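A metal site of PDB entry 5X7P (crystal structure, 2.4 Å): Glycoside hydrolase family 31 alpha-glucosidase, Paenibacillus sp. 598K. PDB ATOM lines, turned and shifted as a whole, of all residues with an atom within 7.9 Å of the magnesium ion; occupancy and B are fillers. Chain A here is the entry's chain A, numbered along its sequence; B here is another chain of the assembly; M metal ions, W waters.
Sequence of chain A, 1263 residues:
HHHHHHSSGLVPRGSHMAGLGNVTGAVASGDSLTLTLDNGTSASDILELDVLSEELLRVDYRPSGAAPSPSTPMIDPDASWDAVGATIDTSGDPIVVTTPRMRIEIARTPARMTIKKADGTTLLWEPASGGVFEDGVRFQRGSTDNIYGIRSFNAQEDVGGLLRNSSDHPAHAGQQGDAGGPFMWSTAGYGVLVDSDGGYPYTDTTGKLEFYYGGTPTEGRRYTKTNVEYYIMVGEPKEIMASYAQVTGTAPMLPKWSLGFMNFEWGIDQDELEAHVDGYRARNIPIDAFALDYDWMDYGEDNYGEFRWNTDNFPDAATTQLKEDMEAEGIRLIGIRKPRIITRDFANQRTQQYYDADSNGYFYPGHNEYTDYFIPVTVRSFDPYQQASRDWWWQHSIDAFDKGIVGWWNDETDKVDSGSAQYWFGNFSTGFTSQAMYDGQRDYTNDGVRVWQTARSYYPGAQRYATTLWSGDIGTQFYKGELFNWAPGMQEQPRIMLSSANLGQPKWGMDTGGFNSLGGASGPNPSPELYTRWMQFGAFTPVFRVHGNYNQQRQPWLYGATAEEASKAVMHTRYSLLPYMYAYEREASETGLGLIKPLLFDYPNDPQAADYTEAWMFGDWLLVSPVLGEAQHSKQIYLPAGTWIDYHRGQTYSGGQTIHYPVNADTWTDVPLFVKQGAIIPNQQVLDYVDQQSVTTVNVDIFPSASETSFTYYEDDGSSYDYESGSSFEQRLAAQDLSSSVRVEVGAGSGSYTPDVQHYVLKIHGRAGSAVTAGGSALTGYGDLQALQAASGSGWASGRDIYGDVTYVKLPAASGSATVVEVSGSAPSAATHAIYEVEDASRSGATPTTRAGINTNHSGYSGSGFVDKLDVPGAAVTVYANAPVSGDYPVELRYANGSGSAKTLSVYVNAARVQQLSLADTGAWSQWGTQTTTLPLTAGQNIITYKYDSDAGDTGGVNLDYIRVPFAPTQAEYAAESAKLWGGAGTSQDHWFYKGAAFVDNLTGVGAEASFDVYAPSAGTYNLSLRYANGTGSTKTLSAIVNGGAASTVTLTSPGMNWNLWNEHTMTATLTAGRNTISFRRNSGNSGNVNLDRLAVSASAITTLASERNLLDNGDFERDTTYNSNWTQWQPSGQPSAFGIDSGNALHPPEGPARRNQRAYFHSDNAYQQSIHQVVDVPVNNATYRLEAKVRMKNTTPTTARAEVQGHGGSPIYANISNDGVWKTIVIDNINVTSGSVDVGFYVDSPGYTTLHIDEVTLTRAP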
ATOM      1  N   ASN A 263      32.478 -27.112  15.770  1.00  0.00           N
ATOM      2  CA  ASN A 263      31.174 -26.867  15.160  1.00  0.00           C
ATOM      3  C   ASN A 263      30.438 -25.871  16.060  1.00  0.00           C
ATOM      4  O   ASN A 263      29.979 -26.255  17.128  1.00  0.00           O
ATOM      5  CB  ASN A 263      30.404 -28.210  15.098  1.00  0.00           C
ATOM      6  CG  ASN A 263      29.208 -28.215  14.139  1.00  0.00           C
ATOM      7  OD1 ASN A 263      28.940 -29.267  13.556  1.00  0.00           O
ATOM      8  ND2 ASN A 263      28.479 -27.100  14.004  1.00  0.00           N
ATOM      9  N   PHE A 264      30.338 -24.592  15.645  1.00  0.00           N
ATOM     10  CA  PHE A 264      29.547 -23.603  16.392  1.00  0.00           C
ATOM     11  C   PHE A 264      28.129 -23.759  15.887  1.00  0.00           C
ATOM     12  O   PHE A 264      27.904 -24.116  14.684  1.00  0.00           O
ATOM     13  CB  PHE A 264      30.050 -22.178  16.182  1.00  0.00           C
ATOM     14  CG  PHE A 264      31.285 -21.831  16.958  1.00  0.00           C
ATOM     15  CD1 PHE A 264      32.432 -22.620  16.879  1.00  0.00           C
ATOM     16  CD2 PHE A 264      31.316 -20.704  17.807  1.00  0.00           C
ATOM     17  CE1 PHE A 264      33.583 -22.304  17.640  1.00  0.00           C
ATOM     18  CE2 PHE A 264      32.460 -20.369  18.527  1.00  0.00           C
ATOM     19  CZ  PHE A 264      33.588 -21.190  18.467  1.00  0.00           C
ATOM     20  N   GLU A 265      27.154 -23.584  16.785  1.00  0.00           N
ATOM     21  CA  GLU A 265      25.757 -23.764  16.380  1.00  0.00           C
ATOM     22  C   GLU A 265      24.752 -23.025  17.252  1.00  0.00           C
ATOM     23  O   GLU A 265      24.823 -23.054  18.469  1.00  0.00           O
ATOM     24  CB  GLU A 265      25.375 -25.251  16.284  1.00  0.00           C
ATOM     25  CG  GLU A 265      24.101 -25.539  15.476  1.00  0.00           C
ATOM     26  CD  GLU A 265      23.914 -27.016  15.109  1.00  0.00           C
ATOM     27  OE1 GLU A 265      24.908 -27.720  14.767  1.00  0.00           O
ATOM     28  OE2 GLU A 265      22.745 -27.496  15.136  1.00  0.00           O
ATOM     29  N   TRP A 266      23.786 -22.424  16.575  1.00  0.00           N
ATOM     30  CA  TRP A 266      22.646 -21.748  17.172  1.00  0.00           C
ATOM     31  C   TRP A 266      21.400 -22.481  16.675  1.00  0.00           C
ATOM     32  O   TRP A 266      21.089 -22.507  15.477  1.00  0.00           O
ATOM     33  CB  TRP A 266      22.623 -20.282  16.710  1.00  0.00           C
ATOM     34  CG  TRP A 266      21.580 -19.425  17.328  1.00  0.00           C
ATOM     35  CD1 TRP A 266      20.831 -19.699  18.443  1.00  0.00           C
ATOM     36  CD2 TRP A 266      21.258 -18.095  16.942  1.00  0.00           C
ATOM     37  NE1 TRP A 266      20.015 -18.654  18.733  1.00  0.00           N
ATOM     38  CE2 TRP A 266      20.258 -17.643  17.832  1.00  0.00           C
ATOM     39  CE3 TRP A 266      21.696 -17.234  15.926  1.00  0.00           C
ATOM     40  CZ2 TRP A 266      19.692 -16.377  17.749  1.00  0.00           C
ATOM     41  CZ3 TRP A 266      21.140 -15.985  15.814  1.00  0.00           C
ATOM     42  CH2 TRP A 266      20.132 -15.558  16.729  1.00  0.00           C
ATOM     43  N   GLY A 267      20.658 -23.021  17.628  1.00  0.00           N
ATOM     44  CA  GLY A 267      19.503 -23.836  17.337  1.00  0.00           C
ATOM     45  C   GLY A 267      19.945 -25.264  17.550  1.00  0.00           C
ATOM     46  O   GLY A 267      20.281 -25.948  16.569  1.00  0.00           O
ATOM     47  N   ILE A 268      19.927 -25.707  18.812  1.00  0.00           N
ATOM     48  CA  ILE A 268      20.483 -26.990  19.181  1.00  0.00           C
ATOM     49  C   ILE A 268      20.118 -27.389  20.628  1.00  0.00           C
ATOM     50  O   ILE A 268      20.046 -26.548  21.518  1.00  0.00           O
ATOM     51  CB  ILE A 268      21.990 -26.983  18.993  1.00  0.00           C
ATOM     52  CG1 ILE A 268      22.624 -28.354  19.280  1.00  0.00           C
ATOM     53  CG2 ILE A 268      22.619 -25.919  19.875  1.00  0.00           C
ATOM     54  CD1 ILE A 268      24.056 -28.517  18.789  1.00  0.00           C
ATOM     55  N   ASP A 269      19.914 -28.680  20.840  1.00  0.00           N
ATOM     56  CA  ASP A 269      19.595 -29.249  22.158  1.00  0.00           C
ATOM     57  C   ASP A 269      20.394 -30.550  22.330  1.00  0.00           C
ATOM     58  O   ASP A 269      21.085 -30.960  21.391  1.00  0.00           O
ATOM     59  CB  ASP A 269      18.041 -29.456  22.342  1.00  0.00           C
ATOM     60  CG  ASP A 269      17.419 -30.503  21.367  1.00  0.00           C
ATOM     61  OD1 ASP A 269      18.114 -31.293  20.721  1.00  0.00           O
ATOM     62  OD2 ASP A 269      16.197 -30.548  21.233  1.00  0.00           O
ATOM     63  N   GLU A 272      20.164 -33.334  19.599  1.00  0.00           N
ATOM     64  CA  GLU A 272      20.721 -32.924  18.324  1.00  0.00           C
ATOM     65  C   GLU A 272      22.261 -32.945  18.411  1.00  0.00           C
ATOM     66  O   GLU A 272      22.935 -33.505  17.535  1.00  0.00           O
ATOM     67  CB  GLU A 272      20.173 -31.554  17.879  1.00  0.00           C
ATOM     68  CG  GLU A 272      18.818 -31.619  17.156  1.00  0.00           C
ATOM     69  CD  GLU A 272      17.885 -30.414  17.419  1.00  0.00           C
ATOM     70  OE1 GLU A 272      18.364 -29.252  17.595  1.00  0.00           O
ATOM     71  OE2 GLU A 272      16.645 -30.655  17.447  1.00  0.00           O
ATOM     72  N   LEU A 273      22.801 -32.354  19.480  1.00  0.00           N
ATOM     73  CA  LEU A 273      24.210 -32.421  19.801  1.00  0.00           C
ATOM     74  C   LEU A 273      24.742 -33.849  19.662  1.00  0.00           C
ATOM     75  O   LEU A 273      25.693 -34.088  18.951  1.00  0.00           O
ATOM     76  CB  LEU A 273      24.447 -31.887  21.217  1.00  0.00           C
ATOM     77  CG  LEU A 273      25.852 -31.975  21.742  1.00  0.00           C
ATOM     78  CD1 LEU A 273      26.797 -31.140  20.900  1.00  0.00           C
ATOM     79  CD2 LEU A 273      25.872 -31.525  23.185  1.00  0.00           C
ATOM     80  N   HIS A 276      24.695 -35.081  16.141  1.00  0.00           N
ATOM     81  CA  HIS A 276      25.782 -34.450  15.411  1.00  0.00           C
ATOM     82  C   HIS A 276      27.121 -35.117  15.729  1.00  0.00           C
ATOM     83  O   HIS A 276      27.839 -35.445  14.827  1.00  0.00           O
ATOM     84  CB  HIS A 276      25.915 -32.941  15.662  1.00  0.00           C
ATOM     85  CG  HIS A 276      24.711 -32.143  15.307  1.00  0.00           C
ATOM     86  ND1 HIS A 276      23.901 -32.446  14.234  1.00  0.00           N
ATOM     87  CD2 HIS A 276      24.176 -31.031  15.875  1.00  0.00           C
ATOM     88  CE1 HIS A 276      22.920 -31.562  14.155  1.00  0.00           C
ATOM     89  NE2 HIS A 276      23.060 -30.695  15.152  1.00  0.00           N
ATOM     90  N   PHE A 290      32.107 -28.550  20.188  1.00  0.00           N
ATOM     91  CA  PHE A 290      30.924 -27.871  19.755  1.00  0.00           C
ATOM     92  C   PHE A 290      30.824 -26.606  20.594  1.00  0.00           C
ATOM     93  O   PHE A 290      31.178 -26.604  21.779  1.00  0.00           O
ATOM     94  CB  PHE A 290      29.708 -28.754  20.000  1.00  0.00           C
ATOM     95  CG  PHE A 290      29.122 -29.328  18.752  1.00  0.00           C
ATOM     96  CD1 PHE A 290      29.556 -30.545  18.262  1.00  0.00           C
ATOM     97  CD2 PHE A 290      28.142 -28.627  18.068  1.00  0.00           C
ATOM     98  CE1 PHE A 290      28.989 -31.073  17.122  1.00  0.00           C
ATOM     99  CE2 PHE A 290      27.593 -29.146  16.919  1.00  0.00           C
ATOM    100  CZ  PHE A 290      28.014 -30.373  16.447  1.00  0.00           C
ATOM    101  N   ASP A 295      20.951 -21.334  23.233  1.00  0.00           N
ATOM    102  CA  ASP A 295      20.405 -22.633  23.645  1.00  0.00           C
ATOM    103  C   ASP A 295      20.977 -23.103  24.992  1.00  0.00           C
ATOM    104  O   ASP A 295      20.251 -23.629  25.825  1.00  0.00           O
ATOM    105  CB  ASP A 295      20.664 -23.703  22.581  1.00  0.00           C
ATOM    106  CG  ASP A 295      20.392 -23.237  21.179  1.00  0.00           C
ATOM    107  OD1 ASP A 295      21.271 -22.544  20.585  1.00  0.00           O
ATOM    108  OD2 ASP A 295      19.322 -23.573  20.634  1.00  0.00           O
ATOM    109  N   ASN B 348      11.174 -24.914  14.381  1.00  0.00           N
ATOM    110  CA  ASN B 348      11.648 -24.922  12.990  1.00  0.00           C
ATOM    111  C   ASN B 348      10.837 -25.789  11.993  1.00  0.00           C
ATOM    112  O   ASN B 348      11.328 -26.064  10.909  1.00  0.00           O
ATOM    113  CB  ASN B 348      13.150 -25.233  12.902  1.00  0.00           C
ATOM    114  CG  ASN B 348      13.818 -24.523  11.730  1.00  0.00           C
ATOM    115  OD1 ASN B 348      13.411 -23.430  11.334  1.00  0.00           O
ATOM    116  ND2 ASN B 348      14.832 -25.149  11.146  1.00  0.00           N
ATOM    117  N   ASN B 549      23.644 -19.118  11.068  1.00  0.00           N
ATOM    118  CA  ASN B 549      22.546 -18.377  11.683  1.00  0.00           C
ATOM    119  C   ASN B 549      21.601 -19.338  12.424  1.00  0.00           C
ATOM    120  O   ASN B 549      21.844 -20.571  12.475  1.00  0.00           O
ATOM    121  CB  ASN B 549      21.801 -17.473  10.656  1.00  0.00           C
ATOM    122  CG  ASN B 549      21.288 -16.166  11.274  1.00  0.00           C
ATOM    123  OD1 ASN B 549      21.048 -16.125  12.444  1.00  0.00           O
ATOM    124  ND2 ASN B 549      21.130 -15.134  10.482  1.00  0.00           N
ATOM    125  N   TYR B 550      20.571 -18.751  13.047  1.00  0.00           N
ATOM    126  CA  TYR B 550      19.613 -19.504  13.835  1.00  0.00           C
ATOM    127  C   TYR B 550      19.047 -20.672  13.024  1.00  0.00           C
ATOM    128  O   TYR B 550      18.505 -20.457  11.934  1.00  0.00           O
ATOM    129  CB  TYR B 550      18.455 -18.593  14.303  1.00  0.00           C
ATOM    130  CG  TYR B 550      17.498 -19.269  15.244  1.00  0.00           C
ATOM    131  CD1 TYR B 550      17.954 -19.780  16.467  1.00  0.00           C
ATOM    132  CD2 TYR B 550      16.117 -19.430  14.934  1.00  0.00           C
ATOM    133  CE1 TYR B 550      17.086 -20.392  17.378  1.00  0.00           C
ATOM    134  CE2 TYR B 550      15.233 -20.049  15.830  1.00  0.00           C
ATOM    135  CZ  TYR B 550      15.731 -20.528  17.046  1.00  0.00           C
ATOM    136  OH  TYR B 550      14.945 -21.152  17.959  1.00  0.00           O
ATOM    137  N   ASN B 551      19.209 -21.877  13.572  1.00  0.00           N
ATOM    138  CA  ASN B 551      18.612 -23.117  13.077  1.00  0.00           C
ATOM    139  C   ASN B 551      19.127 -23.536  11.685  1.00  0.00           C
ATOM    140  O   ASN B 551      18.458 -24.274  10.942  1.00  0.00           O
ATOM    141  CB  ASN B 551      17.060 -23.045  13.114  1.00  0.00           C
ATOM    142  CG  ASN B 551      16.479 -23.498  14.443  1.00  0.00           C
ATOM    143  OD1 ASN B 551      17.111 -24.243  15.203  1.00  0.00           O
ATOM    144  ND2 ASN B 551      15.269 -23.067  14.717  1.00  0.00           N
ATOM    145  N   GLN B 552      20.317 -23.023  11.367  1.00  0.00           N
ATOM    146  CA  GLN B 552      21.037 -23.383  10.167  1.00  0.00           C
ATOM    147  C   GLN B 552      22.037 -24.441  10.606  1.00  0.00           C
ATOM    148  O   GLN B 552      22.463 -24.471  11.784  1.00  0.00           O
ATOM    149  CB  GLN B 552      21.755 -22.181   9.543  1.00  0.00           C
ATOM    150  CG  GLN B 552      20.810 -21.148   8.960  1.00  0.00           C
ATOM    151  CD  GLN B 552      21.528 -20.158   8.046  1.00  0.00           C
ATOM    152  OE1 GLN B 552      22.717 -19.971   8.175  1.00  0.00           O
ATOM    153  NE2 GLN B 552      20.793 -19.528   7.126  1.00  0.00           N
ATOM    154  N   GLN B 553      22.390 -25.307   9.669  1.00  0.00           N
ATOM    155  CA  GLN B 553      23.194 -26.470   9.953  1.00  0.00           C
ATOM    156  C   GLN B 553      24.453 -26.454   9.114  1.00  0.00           C
ATOM    157  O   GLN B 553      24.448 -26.119   7.912  1.00  0.00           O
ATOM    158  CB  GLN B 553      22.351 -27.745   9.685  1.00  0.00           C
ATOM    159  CG  GLN B 553      21.154 -27.939  10.611  1.00  0.00           C
ATOM    160  CD  GLN B 553      21.543 -27.997  12.101  1.00  0.00           C
ATOM    161  OE1 GLN B 553      20.816 -27.508  12.953  1.00  0.00           O
ATOM    162  NE2 GLN B 553      22.706 -28.557  12.407  1.00  0.00           N
ATOM    163  N   ARG B 554      25.553 -26.846   9.750  1.00  0.00           N
ATOM    164  CA  ARG B 554      26.885 -26.789   9.092  1.00  0.00           C
ATOM    165  C   ARG B 554      27.682 -28.120   9.082  1.00  0.00           C
ATOM    166  O   ARG B 554      28.900 -28.130   8.795  1.00  0.00           O
ATOM    167  CB  ARG B 554      27.724 -25.623   9.703  1.00  0.00           C
ATOM    168  CG  ARG B 554      27.186 -24.217   9.392  1.00  0.00           C
ATOM    169  CD  ARG B 554      27.389 -23.788   7.930  1.00  0.00           C
ATOM    170  NE  ARG B 554      26.953 -22.413   7.687  1.00  0.00           N
ATOM    171  CZ  ARG B 554      25.717 -22.025   7.359  1.00  0.00           C
ATOM    172  NH1 ARG B 554      24.726 -22.915   7.157  1.00  0.00           N
ATOM    173  NH2 ARG B 554      25.473 -20.717   7.213  1.00  0.00           N
ATOM    174  N   GLN B 555      27.008 -29.229   9.329  1.00  0.00           N
ATOM    175  CA  GLN B 555      27.674 -30.535   9.288  1.00  0.00           C
ATOM    176  C   GLN B 555      27.955 -30.845   7.790  1.00  0.00           C
ATOM    177  O   GLN B 555      27.152 -30.537   6.924  1.00  0.00           O
ATOM    178  CB  GLN B 555      26.836 -31.654   9.959  1.00  0.00           C
ATOM    179  CG  GLN B 555      26.671 -31.527  11.494  1.00  0.00           C
ATOM    180  CD  GLN B 555      25.728 -30.426  11.934  1.00  0.00           C
ATOM    181  OE1 GLN B 555      24.702 -30.246  11.309  1.00  0.00           O
ATOM    182  NE2 GLN B 555      26.082 -29.687  13.011  1.00  0.00           N
HETATM  183 MG    MG M   1      20.660 -27.032  14.818  1.00  0.00          MG
HETATM  184  O   HOH W   1      18.758 -26.657  14.544  1.00  0.00           O
HETATM  185  O   HOH W   2      20.048 -28.989  15.628  1.00  0.00           O
HETATM  186  O   HOH W   3      20.994 -25.070  14.120  1.00  0.00           O
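The backbone NH (N) of Gly 267 is in hydrogen-bond range of the side-chain carboxylate (OD1) of Asp 295, at 3.1 Å.
The side-chain amide nitrogen (NE2) of Gln 553 of chain B lies close to a ring nitrogen (NE2) of His 276, at 3.5 Å.
The side-chain amide nitrogen of Gln 553 of chain B lies within hydrogen-bond range of the side-chain amide oxygen of Gln 555 of chain B (2.8 Å).
The side-chain amide nitrogen (NE2) of Gln 555 of chain B sits at hydrogen-bond distance from the side-chain carboxylate (OE1) of Glu 265, at 2.9 Å.
NE2 of His 276 sits close to OE2 of Glu 265 (3.2 Å).
The nearest printed residue that does not touch the magnesium ion is Glu 272 (4.2 Å).
The magnesium ion is bound by the side-chain amide oxygen (OE1) of Gln 553 of chain B (1.9 Å).
Water W1 is bound to the magnesium ion (2.0 Å).
O of Gly 267 binds the magnesium ion (2.1 Å).
The magnesium ion is bound by water W3 (2.1 Å).
OE2 of Glu 265 is bound to the magnesium ion (2.2 Å).
The magnesium ion is bound by water W2 (2.2 Å).
The magnesium ion has six donor atoms within binding distance.
Water W3 bridges the backbone carbonyl oxygen of Gln 552 of chain B (2.8 Å) and the backbone carbonyl oxygen of Trp 266 (2.9 Å).
Water W2 lies within hydrogen-bond range of OE1 of Glu 272 (2.6 Å) and NE2 of His 276 (3.5 Å).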
